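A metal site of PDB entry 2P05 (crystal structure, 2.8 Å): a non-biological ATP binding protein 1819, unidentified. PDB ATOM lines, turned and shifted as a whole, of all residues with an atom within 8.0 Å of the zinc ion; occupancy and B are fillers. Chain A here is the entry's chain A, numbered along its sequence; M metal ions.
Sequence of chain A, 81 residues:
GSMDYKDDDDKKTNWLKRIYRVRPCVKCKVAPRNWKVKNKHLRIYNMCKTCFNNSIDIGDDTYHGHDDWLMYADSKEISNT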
ATOM      1  N   PRO A  24     -11.500 -17.832 -27.003  1.00  0.00           N
ATOM      2  CA  PRO A  24     -12.101 -16.993 -25.971  1.00  0.00           C
ATOM      3  C   PRO A  24     -12.815 -17.829 -24.896  1.00  0.00           C
ATOM      4  O   PRO A  24     -12.888 -19.048 -24.959  1.00  0.00           O
ATOM      5  CB  PRO A  24     -13.151 -16.187 -26.723  1.00  0.00           C
ATOM      6  CG  PRO A  24     -13.057 -16.594 -28.197  1.00  0.00           C
ATOM      7  CD  PRO A  24     -12.231 -17.810 -28.278  1.00  0.00           C
ATOM      8  N   CYS A  25     -13.320 -17.159 -23.880  1.00  0.00           N
ATOM      9  CA  CYS A  25     -14.096 -17.831 -22.853  1.00  0.00           C
ATOM     10  C   CYS A  25     -15.304 -18.545 -23.491  1.00  0.00           C
ATOM     11  O   CYS A  25     -15.979 -17.967 -24.342  1.00  0.00           O
ATOM     12  CB  CYS A  25     -14.588 -16.772 -21.894  1.00  0.00           C
ATOM     13  SG  CYS A  25     -15.531 -17.472 -20.595  1.00  0.00           S
ATOM     14  N   VAL A  26     -15.571 -19.793 -23.079  1.00  0.00           N
ATOM     15  CA  VAL A  26     -16.754 -20.553 -23.584  1.00  0.00           C
ATOM     16  C   VAL A  26     -18.080 -19.958 -23.111  1.00  0.00           C
ATOM     17  O   VAL A  26     -19.101 -20.091 -23.787  1.00  0.00           O
ATOM     18  CB  VAL A  26     -16.749 -22.083 -23.236  1.00  0.00           C
ATOM     19  CG1 VAL A  26     -15.635 -22.862 -24.019  1.00  0.00           C
ATOM     20  CG2 VAL A  26     -16.652 -22.314 -21.748  1.00  0.00           C
ATOM     21  N   LYS A  27     -18.081 -19.291 -21.980  1.00  0.00           N
ATOM     22  CA  LYS A  27     -19.281 -18.720 -21.492  1.00  0.00           C
ATOM     23  C   LYS A  27     -19.537 -17.364 -22.098  1.00  0.00           C
ATOM     24  O   LYS A  27     -20.580 -17.135 -22.618  1.00  0.00           O
ATOM     25  CB  LYS A  27     -19.259 -18.667 -19.956  1.00  0.00           C
ATOM     26  CG  LYS A  27     -20.623 -18.329 -19.249  1.00  0.00           C
ATOM     27  CD  LYS A  27     -21.770 -19.199 -19.715  1.00  0.00           C
ATOM     28  CE  LYS A  27     -22.940 -19.121 -18.791  1.00  0.00           C
ATOM     29  NZ  LYS A  27     -24.143 -19.616 -19.520  1.00  0.00           N
ATOM     30  N   CYS A  28     -18.605 -16.425 -22.056  1.00  0.00           N
ATOM     31  CA  CYS A  28     -18.951 -15.098 -22.509  1.00  0.00           C
ATOM     32  C   CYS A  28     -18.491 -14.808 -23.919  1.00  0.00           C
ATOM     33  O   CYS A  28     -18.829 -13.779 -24.456  1.00  0.00           O
ATOM     34  CB  CYS A  28     -18.396 -14.018 -21.569  1.00  0.00           C
ATOM     35  SG  CYS A  28     -16.572 -13.874 -21.551  1.00  0.00           S
ATOM     36  N   LYS A  29     -17.654 -15.670 -24.493  1.00  0.00           N
ATOM     37  CA  LYS A  29     -17.286 -15.567 -25.895  1.00  0.00           C
ATOM     38  C   LYS A  29     -16.455 -14.319 -26.272  1.00  0.00           C
ATOM     39  O   LYS A  29     -16.083 -14.135 -27.416  1.00  0.00           O
ATOM     40  CB  LYS A  29     -18.550 -15.709 -26.741  1.00  0.00           C
ATOM     41  CG  LYS A  29     -18.988 -17.133 -26.813  1.00  0.00           C
ATOM     42  CD  LYS A  29     -20.449 -17.268 -27.176  1.00  0.00           C
ATOM     43  CE  LYS A  29     -21.011 -18.693 -26.796  1.00  0.00           C
ATOM     44  NZ  LYS A  29     -19.950 -19.803 -26.860  1.00  0.00           N
ATOM     45  N   VAL A  30     -16.153 -13.478 -25.300  1.00  0.00           N
ATOM     46  CA  VAL A  30     -15.358 -12.270 -25.501  1.00  0.00           C
ATOM     47  C   VAL A  30     -13.963 -12.333 -24.797  1.00  0.00           C
ATOM     48  O   VAL A  30     -12.943 -12.330 -25.501  1.00  0.00           O
ATOM     49  CB  VAL A  30     -16.074 -11.016 -25.001  1.00  0.00           C
ATOM     50  CG1 VAL A  30     -15.185  -9.842 -25.203  1.00  0.00           C
ATOM     51  CG2 VAL A  30     -17.395 -10.798 -25.711  1.00  0.00           C
ATOM     52  N   ALA A  31     -13.888 -12.378 -23.451  1.00  0.00           N
ATOM     53  CA  ALA A  31     -12.629 -12.365 -22.696  1.00  0.00           C
ATOM     54  C   ALA A  31     -11.777 -13.614 -22.946  1.00  0.00           C
ATOM     55  O   ALA A  31     -12.320 -14.658 -23.293  1.00  0.00           O
ATOM     56  CB  ALA A  31     -12.925 -12.232 -21.233  1.00  0.00           C
ATOM     57  N   PRO A  32     -10.430 -13.509 -22.835  1.00  0.00           N
ATOM     58  CA  PRO A  32      -9.582 -14.721 -22.907  1.00  0.00           C
ATOM     59  C   PRO A  32      -9.747 -15.614 -21.669  1.00  0.00           C
ATOM     60  O   PRO A  32     -10.278 -15.146 -20.684  1.00  0.00           O
ATOM     61  CB  PRO A  32      -8.140 -14.156 -23.010  1.00  0.00           C
ATOM     62  CG  PRO A  32      -8.213 -12.784 -22.424  1.00  0.00           C
ATOM     63  CD  PRO A  32      -9.626 -12.268 -22.686  1.00  0.00           C
ATOM     64  N   ARG A  33      -9.311 -16.880 -21.752  1.00  0.00           N
ATOM     65  CA  ARG A  33      -9.527 -17.898 -20.722  1.00  0.00           C
ATOM     66  C   ARG A  33      -8.591 -17.686 -19.561  1.00  0.00           C
ATOM     67  O   ARG A  33      -7.626 -16.944 -19.693  1.00  0.00           O
ATOM     68  CB  ARG A  33      -9.313 -19.296 -21.325  1.00  0.00           C
ATOM     69  CG  ARG A  33     -10.541 -19.768 -22.019  1.00  0.00           C
ATOM     70  CD  ARG A  33     -10.359 -20.200 -23.390  1.00  0.00           C
ATOM     71  NE  ARG A  33     -10.526 -21.644 -23.485  1.00  0.00           N
ATOM     72  CZ  ARG A  33     -11.344 -22.276 -24.336  1.00  0.00           C
ATOM     73  NH1 ARG A  33     -12.114 -21.632 -25.229  1.00  0.00           N
ATOM     74  NH2 ARG A  33     -11.363 -23.599 -24.308  1.00  0.00           N
ATOM     75  N   ASN A  34      -8.834 -18.301 -18.422  1.00  0.00           N
ATOM     76  CA  ASN A  34      -7.923 -18.183 -17.322  1.00  0.00           C
ATOM     77  C   ASN A  34      -6.983 -19.300 -17.560  1.00  0.00           C
ATOM     78  O   ASN A  34      -7.289 -20.194 -18.342  1.00  0.00           O
ATOM     79  CB  ASN A  34      -8.657 -18.405 -16.014  1.00  0.00           C
ATOM     80  CG  ASN A  34      -7.786 -18.134 -14.819  1.00  0.00           C
ATOM     81  OD1 ASN A  34      -6.711 -17.557 -14.947  1.00  0.00           O
ATOM     82  ND2 ASN A  34      -8.245 -18.534 -13.657  1.00  0.00           N
ATOM     83  N   ASN A  46     -11.448 -23.504 -19.152  1.00  0.00           N
ATOM     84  CA  ASN A  46     -12.479 -23.157 -20.131  1.00  0.00           C
ATOM     85  C   ASN A  46     -12.981 -21.737 -20.082  1.00  0.00           C
ATOM     86  O   ASN A  46     -13.434 -21.254 -21.097  1.00  0.00           O
ATOM     87  CB  ASN A  46     -13.699 -24.097 -20.047  1.00  0.00           C
ATOM     88  CG  ASN A  46     -13.372 -25.507 -20.446  1.00  0.00           C
ATOM     89  OD1 ASN A  46     -13.196 -25.789 -21.616  1.00  0.00           O
ATOM     90  ND2 ASN A  46     -13.275 -26.389 -19.497  1.00  0.00           N
ATOM     91  N   MET A  47     -12.959 -21.084 -18.926  1.00  0.00           N
ATOM     92  CA  MET A  47     -13.603 -19.774 -18.778  1.00  0.00           C
ATOM     93  C   MET A  47     -12.695 -18.674 -18.208  1.00  0.00           C
ATOM     94  O   MET A  47     -11.802 -18.951 -17.431  1.00  0.00           O
ATOM     95  CB  MET A  47     -14.806 -19.885 -17.837  1.00  0.00           C
ATOM     96  CG  MET A  47     -16.044 -20.624 -18.402  1.00  0.00           C
ATOM     97  SD  MET A  47     -17.468 -20.584 -17.274  1.00  0.00           S
ATOM     98  CE  MET A  47     -16.878 -21.659 -15.961  1.00  0.00           C
ATOM     99  N   CYS A  48     -12.989 -17.403 -18.526  1.00  0.00           N
ATOM    100  CA  CYS A  48     -12.329 -16.302 -17.853  1.00  0.00           C
ATOM    101  C   CYS A  48     -12.488 -16.418 -16.324  1.00  0.00           C
ATOM    102  O   CYS A  48     -13.165 -17.306 -15.861  1.00  0.00           O
ATOM    103  CB  CYS A  48     -12.812 -14.973 -18.431  1.00  0.00           C
ATOM    104  SG  CYS A  48     -14.469 -14.347 -17.980  1.00  0.00           S
ATOM    105  N   LYS A  49     -11.807 -15.604 -15.525  1.00  0.00           N
ATOM    106  CA  LYS A  49     -12.005 -15.725 -14.090  1.00  0.00           C
ATOM    107  C   LYS A  49     -13.406 -15.225 -13.707  1.00  0.00           C
ATOM    108  O   LYS A  49     -13.978 -15.697 -12.717  1.00  0.00           O
ATOM    109  CB  LYS A  49     -10.953 -14.924 -13.308  1.00  0.00           C
ATOM    110  CG  LYS A  49     -10.918 -15.202 -11.790  1.00  0.00           C
ATOM    111  CD  LYS A  49     -10.168 -16.475 -11.485  1.00  0.00           C
ATOM    112  CE  LYS A  49     -10.637 -17.170 -10.204  1.00  0.00           C
ATOM    113  NZ  LYS A  49     -10.473 -16.242  -9.047  1.00  0.00           N
ATOM    114  N   THR A  50     -13.943 -14.240 -14.445  1.00  0.00           N
ATOM    115  CA  THR A  50     -15.129 -13.582 -13.968  1.00  0.00           C
ATOM    116  C   THR A  50     -16.277 -14.515 -14.240  1.00  0.00           C
ATOM    117  O   THR A  50     -17.161 -14.633 -13.392  1.00  0.00           O
ATOM    118  CB  THR A  50     -15.395 -12.132 -14.523  1.00  0.00           C
ATOM    119  OG1 THR A  50     -15.122 -12.089 -15.922  1.00  0.00           O
ATOM    120  CG2 THR A  50     -14.468 -11.091 -13.878  1.00  0.00           C
ATOM    121  N   CYS A  51     -16.267 -15.226 -15.375  1.00  0.00           N
ATOM    122  CA  CYS A  51     -17.335 -16.168 -15.658  1.00  0.00           C
ATOM    123  C   CYS A  51     -17.255 -17.370 -14.793  1.00  0.00           C
ATOM    124  O   CYS A  51     -18.281 -17.969 -14.531  1.00  0.00           O
ATOM    125  CB  CYS A  51     -17.348 -16.617 -17.091  1.00  0.00           C
ATOM    126  SG  CYS A  51     -17.936 -15.329 -18.237  1.00  0.00           S
ATOM    127  N   PHE A  52     -16.055 -17.763 -14.367  1.00  0.00           N
ATOM    128  CA  PHE A  52     -15.938 -18.950 -13.510  1.00  0.00           C
ATOM    129  C   PHE A  52     -16.525 -18.666 -12.157  1.00  0.00           C
ATOM    130  O   PHE A  52     -17.376 -19.431 -11.723  1.00  0.00           O
ATOM    131  CB  PHE A  52     -14.522 -19.436 -13.333  1.00  0.00           C
ATOM    132  CG  PHE A  52     -14.387 -20.642 -12.427  1.00  0.00           C
ATOM    133  CD1 PHE A  52     -14.792 -21.903 -12.857  1.00  0.00           C
ATOM    134  CD2 PHE A  52     -13.780 -20.523 -11.168  1.00  0.00           C
ATOM    135  CE1 PHE A  52     -14.653 -23.024 -12.014  1.00  0.00           C
ATOM    136  CE2 PHE A  52     -13.631 -21.615 -10.325  1.00  0.00           C
ATOM    137  CZ  PHE A  52     -14.067 -22.876 -10.744  1.00  0.00           C
HETATM  138 ZN    ZN M   1     -16.016 -15.318 -19.793  1.00  0.00          ZN
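The zinc ion is bound by the side-chain sulfur (SG) of Cys 28 (2.3 Å), the side-chain sulfur (SG) of Cys 25 (2.3 Å), the side-chain sulfur (SG) of Cys 51 (2.5 Å) and the side-chain sulfur (SG) of Cys 48 (2.6 Å). The zinc ion has four donor atoms within binding distance.
The backbone NH of Val 30 lies close to the side-chain sulfur of Cys 28 (3.8 Å). The backbone NH (N) of Ala 31 lies close to the side-chain sulfur (SG) of Cys 28. SG of Cys 25 sits close to N of Lys 27, 3.4 Å away. SG of Cys 48 sits close to OG1 of Thr 50, 3.1 Å away. N of Cys 25 lies within hydrogen-bond range of O of Ala 31 (2.8 Å).
Along chain A the residues within 4 Å of the zinc ion span positions 25 to 51.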
